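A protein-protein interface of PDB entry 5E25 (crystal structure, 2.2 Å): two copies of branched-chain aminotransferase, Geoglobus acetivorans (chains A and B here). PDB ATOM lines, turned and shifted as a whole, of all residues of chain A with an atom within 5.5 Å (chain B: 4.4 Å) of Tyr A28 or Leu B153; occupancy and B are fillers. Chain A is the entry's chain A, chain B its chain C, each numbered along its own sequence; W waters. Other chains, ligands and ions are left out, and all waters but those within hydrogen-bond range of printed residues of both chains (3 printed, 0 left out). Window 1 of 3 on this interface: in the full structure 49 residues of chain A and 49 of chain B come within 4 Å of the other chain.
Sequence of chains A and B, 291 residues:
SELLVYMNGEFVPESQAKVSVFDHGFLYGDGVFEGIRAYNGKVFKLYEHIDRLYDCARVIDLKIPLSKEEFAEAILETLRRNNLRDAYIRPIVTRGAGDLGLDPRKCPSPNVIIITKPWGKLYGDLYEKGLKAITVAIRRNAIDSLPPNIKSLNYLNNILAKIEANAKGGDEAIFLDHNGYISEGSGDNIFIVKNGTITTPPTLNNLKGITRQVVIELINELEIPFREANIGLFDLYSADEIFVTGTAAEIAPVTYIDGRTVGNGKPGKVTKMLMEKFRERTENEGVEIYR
Thr B94 touches Phe A26 (CG2 to CZ, 3.7 Å). O of Phe A26 touches CD1 of Leu B153, 3.5 Å away. Leu A27 touches Ile B92 (CD2 to CD1, 3.8 Å). O of Leu A27 touches CD2 of Leu B153 (3.3 Å). Ile B159 touches Tyr A28 (CD1 to CB, 3.5 Å). CD2 of Leu B156 touches O of Gly A29, at 3.5 Å. OD1 of Asp A30 touches CD1 of Leu B156 (3.5 Å). OD2 of Asp A30 touches CD1 of Ile B159, at 3.6 Å. Leu A102 touches Tyr B155. Ile B159 touches Leu A102 (CG1 to O, 3.8 Å).
Hydrophobic or aromatic side chains of chain A that line the printed part of chain B: Phe A26, Leu A27, Tyr A28, Leu A102 and Leu A156. Along chain A the printed residues that touch a printed residue of chain B span positions 26 to 156. Among the printed residues, 20 pairs touch across the chains.
Gly A29 touches Leu B156, but with the chains exchanged Leu A156 does not touch Gly B29 (4.3 Å). Asn B154 touches its own counterpart, Asn A154. Asn A154 touches Leu B156, and with the chains exchanged Leu A156 touches Asn B154. Of the 20 pairs that touch across the chains among the printed residues, 3 have their exchanged pair printed and touching as well.
The backbone NH (N) of Leu A156 lies close to the side-chain amide nitrogen (ND2) of Asn B154 (2.9 Å). The backbone carbonyl oxygen (O) of Leu B153 lies within hydrogen-bond range of the backbone NH (N) of Gly A29 (3.0 Å). NH1 of Arg B90 lies within hydrogen-bond range of OH of Tyr A28, at 3.1 Å. The side-chain amide nitrogen (ND2) of Asn A154 lies close to the backbone carbonyl oxygen (O) of Asn B154, 3.4 Å away. The backbone NH of Tyr B155 sits close to the side-chain amide nitrogen of Asn A154, 3.2 Å away. The side-chain amide nitrogen (ND2) of Asn A154 sits close to the backbone NH (N) of Leu B156 (2.9 Å). The backbone carbonyl oxygen (O) of Tyr A28 lies close to the backbone carbonyl oxygen (O) of Leu B153 (3.2 Å). The backbone NH (N) of Tyr B155 is in hydrogen-bond range of the backbone carbonyl oxygen (O) of Tyr A28.
O of Leu A100 is in hydrogen-bond range of OH of Tyr A28 (2.5 Å). The backbone carbonyl oxygen (O) of Gly A29 sits close to the side-chain amide oxygen (OD1) of Asn A154 (2.8 Å). The side-chain amide oxygen of Asn B154 lies close to the backbone carbonyl oxygen of Gly B29 (2.8 Å). The side-chain hydroxyl of Ser B152 lies within hydrogen-bond range of the backbone NH of Asn B154 (2.8 Å). The backbone carbonyl oxygen (O) of Tyr A28 lies close to the side-chain amide oxygen (OD1) of Asn A154 (3.1 Å). The backbone carbonyl oxygen of His A24 sits at hydrogen-bond distance from the backbone NH of Gly A29, 3.4 Å away.
Printed residues of chain B within 4 Å of Tyr A28: Arg B90, Leu B153, Tyr B155, Leu B156 and Ile B159. Leu B153 touches four residues of chain A. Of the printed residues of chain A, Tyr B155 touches Tyr A28, Leu A102 and Asn A154. Of the printed residues of chain B, Gly A29 touches Leu B153 (3.0 Å) and Leu B156 (3.5 Å). Leu A100 touches none of the printed residues of chain B. His A24 touches none of the printed residues of chain B.
Water W3 lies within hydrogen-bond range of the backbone carbonyl oxygen (O) of Asn B154 (2.6 Å), the side-chain amide nitrogen (ND2) of Asn A154 (2.8 Å) and the backbone NH (N) of Leu B156 (3.2 Å). Water W1 lies within hydrogen-bond range of NH1 of Arg B90 and O of Leu A27. Water W2 lies within hydrogen-bond range of O of Asn A154 (2.8 Å), ND2 of Asn B154 (2.8 Å) and N of Leu A156 (3.4 Å).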
ATOM      1  N   ASP A  23     -17.172 -10.458 -23.607  1.00  0.00           N
ATOM      2  CA  ASP A  23     -16.666 -10.994 -24.853  1.00  0.00           C
ATOM      3  C   ASP A  23     -15.824 -12.208 -24.445  1.00  0.00           C
ATOM      4  O   ASP A  23     -14.952 -12.063 -23.612  1.00  0.00           O
ATOM      5  CB  ASP A  23     -15.719  -9.945 -25.497  1.00  0.00           C
ATOM      6  CG  ASP A  23     -15.318 -10.299 -26.952  1.00  0.00           C
ATOM      7  OD1 ASP A  23     -14.582 -11.248 -27.202  1.00  0.00           O
ATOM      8  OD2 ASP A  23     -15.714  -9.595 -27.856  1.00  0.00           O
ATOM      9  N   HIS A  24     -16.114 -13.360 -25.045  1.00  0.00           N
ATOM     10  CA  HIS A  24     -15.384 -14.610 -24.875  1.00  0.00           C
ATOM     11  C   HIS A  24     -13.912 -14.542 -25.284  1.00  0.00           C
ATOM     12  O   HIS A  24     -13.105 -15.310 -24.769  1.00  0.00           O
ATOM     13  CB  HIS A  24     -16.148 -15.757 -25.517  1.00  0.00           C
ATOM     14  CG  HIS A  24     -17.370 -16.134 -24.749  1.00  0.00           C
ATOM     15  ND1 HIS A  24     -17.923 -17.417 -24.783  1.00  0.00           N
ATOM     16  CD2 HIS A  24     -18.168 -15.391 -23.933  1.00  0.00           C
ATOM     17  CE1 HIS A  24     -18.995 -17.440 -24.005  1.00  0.00           C
ATOM     18  NE2 HIS A  24     -19.190 -16.213 -23.515  1.00  0.00           N
ATOM     19  N   GLY A  25     -13.532 -13.567 -26.109  1.00  0.00           N
ATOM     20  CA  GLY A  25     -12.108 -13.250 -26.284  1.00  0.00           C
ATOM     21  C   GLY A  25     -11.439 -12.750 -24.997  1.00  0.00           C
ATOM     22  O   GLY A  25     -10.246 -12.899 -24.751  1.00  0.00           O
ATOM     23  N   PHE A  26     -12.207 -12.084 -24.177  1.00  0.00           N
ATOM     24  CA  PHE A  26     -11.678 -11.638 -22.896  1.00  0.00           C
ATOM     25  C   PHE A  26     -11.868 -12.718 -21.765  1.00  0.00           C
ATOM     26  O   PHE A  26     -10.939 -12.955 -21.008  1.00  0.00           O
ATOM     27  CB  PHE A  26     -12.291 -10.261 -22.542  1.00  0.00           C
ATOM     28  CG  PHE A  26     -11.826  -9.706 -21.240  1.00  0.00           C
ATOM     29  CD1 PHE A  26     -10.625  -9.048 -21.150  1.00  0.00           C
ATOM     30  CD2 PHE A  26     -12.620  -9.837 -20.093  1.00  0.00           C
ATOM     31  CE1 PHE A  26     -10.176  -8.564 -19.922  1.00  0.00           C
ATOM     32  CE2 PHE A  26     -12.195  -9.338 -18.859  1.00  0.00           C
ATOM     33  CZ  PHE A  26     -10.977  -8.699 -18.779  1.00  0.00           C
ATOM     34  N   LEU A  27     -13.017 -13.398 -21.714  1.00  0.00           N
ATOM     35  CA  LEU A  27     -13.286 -14.406 -20.678  1.00  0.00           C
ATOM     36  C   LEU A  27     -12.373 -15.635 -20.835  1.00  0.00           C
ATOM     37  O   LEU A  27     -11.869 -16.135 -19.830  1.00  0.00           O
ATOM     38  CB  LEU A  27     -14.761 -14.816 -20.645  1.00  0.00           C
ATOM     39  CG  LEU A  27     -15.726 -13.652 -20.328  1.00  0.00           C
ATOM     40  CD1 LEU A  27     -17.198 -14.095 -20.391  1.00  0.00           C
ATOM     41  CD2 LEU A  27     -15.383 -12.860 -19.059  1.00  0.00           C
ATOM     42  N   TYR A  28     -12.121 -16.043 -22.101  1.00  0.00           N
ATOM     43  CA  TYR A  28     -11.555 -17.308 -22.430  1.00  0.00           C
ATOM     44  C   TYR A  28     -10.450 -17.330 -23.473  1.00  0.00           C
ATOM     45  O   TYR A  28     -10.059 -18.447 -23.864  1.00  0.00           O
ATOM     46  CB  TYR A  28     -12.666 -18.254 -22.871  1.00  0.00           C
ATOM     47  CG  TYR A  28     -13.761 -18.375 -21.868  1.00  0.00           C
ATOM     48  CD1 TYR A  28     -13.483 -18.767 -20.527  1.00  0.00           C
ATOM     49  CD2 TYR A  28     -15.071 -18.056 -22.200  1.00  0.00           C
ATOM     50  CE1 TYR A  28     -14.493 -18.857 -19.580  1.00  0.00           C
ATOM     51  CE2 TYR A  28     -16.073 -18.149 -21.245  1.00  0.00           C
ATOM     52  CZ  TYR A  28     -15.777 -18.556 -19.944  1.00  0.00           C
ATOM     53  OH  TYR A  28     -16.765 -18.627 -18.989  1.00  0.00           O
ATOM     54  N   GLY A  29      -9.901 -16.148 -23.844  1.00  0.00           N
ATOM     55  CA  GLY A  29      -8.993 -16.014 -24.990  1.00  0.00           C
ATOM     56  C   GLY A  29      -9.598 -16.750 -26.225  1.00  0.00           C
ATOM     57  O   GLY A  29      -8.871 -17.357 -27.010  1.00  0.00           O
ATOM     58  N   ASP A  30     -10.921 -16.678 -26.421  1.00  0.00           N
ATOM     59  CA  ASP A  30     -11.587 -17.379 -27.527  1.00  0.00           C
ATOM     60  C   ASP A  30     -11.559 -16.456 -28.752  1.00  0.00           C
ATOM     61  O   ASP A  30     -12.518 -15.732 -28.988  1.00  0.00           O
ATOM     62  CB  ASP A  30     -13.048 -17.705 -27.103  1.00  0.00           C
ATOM     63  CG  ASP A  30     -13.705 -18.695 -27.990  1.00  0.00           C
ATOM     64  OD1 ASP A  30     -13.034 -19.157 -28.940  1.00  0.00           O
ATOM     65  OD2 ASP A  30     -14.893 -19.025 -27.711  1.00  0.00           O
ATOM     66  N   LEU A 100     -22.359 -16.573 -19.878  1.00  0.00           N
ATOM     67  CA  LEU A 100     -21.130 -16.418 -19.143  1.00  0.00           C
ATOM     68  C   LEU A 100     -20.225 -17.639 -19.296  1.00  0.00           C
ATOM     69  O   LEU A 100     -18.999 -17.498 -19.362  1.00  0.00           O
ATOM     70  CB  LEU A 100     -21.380 -16.146 -17.683  1.00  0.00           C
ATOM     71  CG  LEU A 100     -20.946 -14.789 -17.142  1.00  0.00           C
ATOM     72  CD1 LEU A 100     -20.902 -14.963 -15.632  1.00  0.00           C
ATOM     73  CD2 LEU A 100     -19.611 -14.255 -17.657  1.00  0.00           C
ATOM     74  N   GLY A 101     -20.845 -18.822 -19.380  1.00  0.00           N
ATOM     75  CA  GLY A 101     -20.173 -20.076 -19.675  1.00  0.00           C
ATOM     76  C   GLY A 101     -19.440 -20.166 -21.027  1.00  0.00           C
ATOM     77  O   GLY A 101     -19.508 -19.246 -21.855  1.00  0.00           O
ATOM     78  N   LEU A 102     -18.754 -21.289 -21.277  1.00  0.00           N
ATOM     79  CA  LEU A 102     -17.767 -21.344 -22.397  1.00  0.00           C
ATOM     80  C   LEU A 102     -18.433 -21.779 -23.737  1.00  0.00           C
ATOM     81  O   LEU A 102     -17.790 -21.810 -24.777  1.00  0.00           O
ATOM     82  CB  LEU A 102     -16.579 -22.241 -21.983  1.00  0.00           C
ATOM     83  CG  LEU A 102     -16.721 -23.752 -22.075  1.00  0.00           C
ATOM     84  CD1 LEU A 102     -15.559 -24.382 -21.317  1.00  0.00           C
ATOM     85  CD2 LEU A 102     -18.041 -24.214 -21.473  1.00  0.00           C
ATOM     86  N   ASN A 154      -4.986 -17.383 -26.804  1.00  0.00           N
ATOM     87  CA  ASN A 154      -4.431 -18.190 -25.682  1.00  0.00           C
ATOM     88  C   ASN A 154      -2.933 -18.215 -25.746  1.00  0.00           C
ATOM     89  O   ASN A 154      -2.336 -19.166 -26.261  1.00  0.00           O
ATOM     90  CB  ASN A 154      -4.994 -19.621 -25.706  1.00  0.00           C
ATOM     91  CG  ASN A 154      -6.358 -19.733 -25.029  1.00  0.00           C
ATOM     92  OD1 ASN A 154      -7.315 -18.887 -25.239  1.00  0.00           O
ATOM     93  ND2 ASN A 154      -6.524 -20.825 -24.278  1.00  0.00           N
ATOM     94  N   LEU A 156      -0.769 -17.656 -22.969  1.00  0.00           N
ATOM     95  CA  LEU A 156      -0.077 -17.816 -21.669  1.00  0.00           C
ATOM     96  C   LEU A 156       1.084 -18.803 -21.718  1.00  0.00           C
ATOM     97  O   LEU A 156       2.055 -18.662 -20.973  1.00  0.00           O
ATOM     98  CB  LEU A 156      -1.095 -18.238 -20.581  1.00  0.00           C
ATOM     99  CG  LEU A 156      -0.754 -17.834 -19.148  1.00  0.00           C
ATOM    100  CD1 LEU A 156      -0.158 -16.436 -18.984  1.00  0.00           C
ATOM    101  CD2 LEU A 156      -2.005 -18.010 -18.283  1.00  0.00           C
ATOM    102  N   GLY B  25      -4.851  -9.268 -21.023  1.00  0.00           N
ATOM    103  CA  GLY B  25      -5.922 -10.185 -20.727  1.00  0.00           C
ATOM    104  C   GLY B  25      -6.729 -10.442 -21.986  1.00  0.00           C
ATOM    105  O   GLY B  25      -7.354 -11.467 -22.134  1.00  0.00           O
ATOM    106  N   GLY B  29      -5.057 -13.660 -23.310  1.00  0.00           N
ATOM    107  CA  GLY B  29      -5.701 -14.329 -22.160  1.00  0.00           C
ATOM    108  C   GLY B  29      -4.796 -14.329 -20.933  1.00  0.00           C
ATOM    109  O   GLY B  29      -4.805 -15.277 -20.129  1.00  0.00           O
ATOM    110  N   GLY B  31      -4.333 -13.540 -17.655  1.00  0.00           N
ATOM    111  CA  GLY B  31      -5.020 -13.194 -16.445  1.00  0.00           C
ATOM    112  C   GLY B  31      -5.589 -14.454 -15.841  1.00  0.00           C
ATOM    113  O   GLY B  31      -5.420 -15.512 -16.429  1.00  0.00           O
ATOM    114  N   VAL B  32      -6.299 -14.335 -14.700  1.00  0.00           N
ATOM    115  CA  VAL B  32      -6.897 -15.476 -13.988  1.00  0.00           C
ATOM    116  C   VAL B  32      -8.315 -15.142 -13.592  1.00  0.00           C
ATOM    117  O   VAL B  32      -8.649 -13.989 -13.533  1.00  0.00           O
ATOM    118  CB  VAL B  32      -6.053 -15.908 -12.759  1.00  0.00           C
ATOM    119  CG1 VAL B  32      -4.730 -16.538 -13.191  1.00  0.00           C
ATOM    120  CG2 VAL B  32      -5.717 -14.720 -11.846  1.00  0.00           C
ATOM    121  N   PHE B  33      -9.131 -16.146 -13.282  1.00  0.00           N
ATOM    122  CA  PHE B  33     -10.486 -15.864 -12.953  1.00  0.00           C
ATOM    123  C   PHE B  33     -10.952 -16.850 -11.899  1.00  0.00           C
ATOM    124  O   PHE B  33     -10.326 -17.878 -11.684  1.00  0.00           O
ATOM    125  CB  PHE B  33     -11.387 -15.894 -14.229  1.00  0.00           C
ATOM    126  CG  PHE B  33     -11.775 -17.273 -14.724  1.00  0.00           C
ATOM    127  CD1 PHE B  33     -10.977 -17.932 -15.688  1.00  0.00           C
ATOM    128  CD2 PHE B  33     -12.962 -17.867 -14.330  1.00  0.00           C
ATOM    129  CE1 PHE B  33     -11.326 -19.187 -16.165  1.00  0.00           C
ATOM    130  CE2 PHE B  33     -13.357 -19.097 -14.852  1.00  0.00           C
ATOM    131  CZ  PHE B  33     -12.536 -19.759 -15.769  1.00  0.00           C
ATOM    132  N   ARG B  90     -17.969 -13.764 -10.858  1.00  0.00           N
ATOM    133  CA  ARG B  90     -16.810 -14.012 -11.706  1.00  0.00           C
ATOM    134  C   ARG B  90     -15.790 -12.890 -11.529  1.00  0.00           C
ATOM    135  O   ARG B  90     -15.791 -11.947 -12.300  1.00  0.00           O
ATOM    136  CB  ARG B  90     -17.237 -14.236 -13.200  1.00  0.00           C
ATOM    137  CG  ARG B  90     -16.142 -14.125 -14.300  1.00  0.00           C
ATOM    138  CD  ARG B  90     -15.160 -15.296 -14.344  1.00  0.00           C
ATOM    139  NE  ARG B  90     -15.935 -16.510 -14.485  1.00  0.00           N
ATOM    140  CZ  ARG B  90     -16.273 -17.073 -15.646  1.00  0.00           C
ATOM    141  NH1 ARG B  90     -15.805 -16.626 -16.820  1.00  0.00           N
ATOM    142  NH2 ARG B  90     -17.059 -18.134 -15.607  1.00  0.00           N
ATOM    143  N   ILE B  92     -11.958 -11.481 -12.021  1.00  0.00           N
ATOM    144  CA  ILE B  92     -10.971 -11.655 -13.029  1.00  0.00           C
ATOM    145  C   ILE B  92      -9.845 -10.696 -12.727  1.00  0.00           C
ATOM    146  O   ILE B  92     -10.095  -9.533 -12.413  1.00  0.00           O
ATOM    147  CB  ILE B  92     -11.557 -11.306 -14.426  1.00  0.00           C
ATOM    148  CG1 ILE B  92     -12.629 -12.320 -14.831  1.00  0.00           C
ATOM    149  CG2 ILE B  92     -10.398 -11.173 -15.456  1.00  0.00           C
ATOM    150  CD1 ILE B  92     -13.585 -11.791 -15.928  1.00  0.00           C
ATOM    151  N   THR B  94      -6.314  -9.234 -14.657  1.00  0.00           N
ATOM    152  CA  THR B  94      -5.570  -9.338 -15.873  1.00  0.00           C
ATOM    153  C   THR B  94      -4.282  -8.634 -15.734  1.00  0.00           C
ATOM    154  O   THR B  94      -4.114  -7.817 -14.850  1.00  0.00           O
ATOM    155  CB  THR B  94      -6.296  -8.689 -17.063  1.00  0.00           C
ATOM    156  OG1 THR B  94      -6.185  -7.276 -16.948  1.00  0.00           O
ATOM    157  CG2 THR B  94      -7.736  -9.117 -17.145  1.00  0.00           C
ATOM    158  N   SER B 152      -6.948 -19.886 -15.579  1.00  0.00           N
ATOM    159  CA  SER B 152      -6.508 -18.705 -16.291  1.00  0.00           C
ATOM    160  C   SER B 152      -7.538 -18.335 -17.372  1.00  0.00           C
ATOM    161  O   SER B 152      -8.484 -19.047 -17.616  1.00  0.00           O
ATOM    162  CB  SER B 152      -5.164 -18.927 -16.966  1.00  0.00           C
ATOM    163  OG  SER B 152      -5.314 -19.542 -18.263  1.00  0.00           O
ATOM    164  N   LEU B 153      -7.305 -17.222 -18.037  1.00  0.00           N
ATOM    165  CA  LEU B 153      -8.222 -16.832 -19.087  1.00  0.00           C
ATOM    166  C   LEU B 153      -7.870 -17.560 -20.385  1.00  0.00           C
ATOM    167  O   LEU B 153      -8.492 -17.253 -21.389  1.00  0.00           O
ATOM    168  CB  LEU B 153      -8.125 -15.306 -19.353  1.00  0.00           C
ATOM    169  CG  LEU B 153      -8.475 -14.337 -18.227  1.00  0.00           C
ATOM    170  CD1 LEU B 153      -8.223 -12.918 -18.726  1.00  0.00           C
ATOM    171  CD2 LEU B 153      -9.906 -14.540 -17.751  1.00  0.00           C
ATOM    172  N   ASN B 154      -6.842 -18.448 -20.400  1.00  0.00           N
ATOM    173  CA  ASN B 154      -6.577 -19.326 -21.572  1.00  0.00           C
ATOM    174  C   ASN B 154      -7.487 -20.517 -21.533  1.00  0.00           C
ATOM    175  O   ASN B 154      -7.075 -21.605 -21.059  1.00  0.00           O
ATOM    176  CB  ASN B 154      -5.128 -19.788 -21.631  1.00  0.00           C
ATOM    177  CG  ASN B 154      -4.226 -18.734 -22.157  1.00  0.00           C
ATOM    178  OD1 ASN B 154      -4.385 -17.497 -21.866  1.00  0.00           O
ATOM    179  ND2 ASN B 154      -3.238 -19.160 -22.921  1.00  0.00           N
ATOM    180  N   TYR B 155      -8.709 -20.347 -22.032  1.00  0.00           N
ATOM    181  CA  TYR B 155      -9.693 -21.441 -21.925  1.00  0.00           C
ATOM    182  C   TYR B 155     -10.024 -22.136 -23.269  1.00  0.00           C
ATOM    183  O   TYR B 155     -11.028 -22.849 -23.431  1.00  0.00           O
ATOM    184  CB  TYR B 155     -10.974 -20.857 -21.325  1.00  0.00           C
ATOM    185  CG  TYR B 155     -11.604 -21.660 -20.219  1.00  0.00           C
ATOM    186  CD1 TYR B 155     -10.899 -21.952 -19.043  1.00  0.00           C
ATOM    187  CD2 TYR B 155     -12.897 -22.101 -20.329  1.00  0.00           C
ATOM    188  CE1 TYR B 155     -11.476 -22.671 -18.027  1.00  0.00           C
ATOM    189  CE2 TYR B 155     -13.480 -22.833 -19.309  1.00  0.00           C
ATOM    190  CZ  TYR B 155     -12.773 -23.114 -18.163  1.00  0.00           C
ATOM    191  OH  TYR B 155     -13.376 -23.823 -17.153  1.00  0.00           O
ATOM    192  N   LEU B 156      -9.135 -21.970 -24.233  1.00  0.00           N
ATOM    193  CA  LEU B 156      -9.441 -22.575 -25.573  1.00  0.00           C
ATOM    194  C   LEU B 156      -9.328 -24.117 -25.616  1.00  0.00           C
ATOM    195  O   LEU B 156     -10.104 -24.768 -26.318  1.00  0.00           O
ATOM    196  CB  LEU B 156      -8.565 -21.903 -26.601  1.00  0.00           C
ATOM    197  CG  LEU B 156      -8.969 -21.648 -28.047  1.00  0.00           C
ATOM    198  CD1 LEU B 156     -10.466 -21.460 -28.273  1.00  0.00           C
ATOM    199  CD2 LEU B 156      -8.185 -20.417 -28.465  1.00  0.00           C
ATOM    200  N   ILE B 159     -12.696 -24.911 -24.506  1.00  0.00           N
ATOM    201  CA  ILE B 159     -13.683 -24.614 -25.629  1.00  0.00           C
ATOM    202  C   ILE B 159     -13.614 -25.671 -26.788  1.00  0.00           C
ATOM    203  O   ILE B 159     -14.668 -26.186 -27.257  1.00  0.00           O
ATOM    204  CB  ILE B 159     -13.534 -23.163 -26.125  1.00  0.00           C
ATOM    205  CG1 ILE B 159     -13.988 -22.224 -24.941  1.00  0.00           C
ATOM    206  CG2 ILE B 159     -14.337 -22.939 -27.447  1.00  0.00           C
ATOM    207  CD1 ILE B 159     -13.426 -20.841 -25.030  1.00  0.00           C
HETATM  208  O   HOH W   1     -13.275 -15.897 -17.254  1.00  0.00           O
HETATM  209  O   HOH W   2      -1.268 -20.742 -24.220  1.00  0.00           O
HETATM  210  O   HOH W   3      -6.472 -23.286 -23.010  1.00  0.00           O
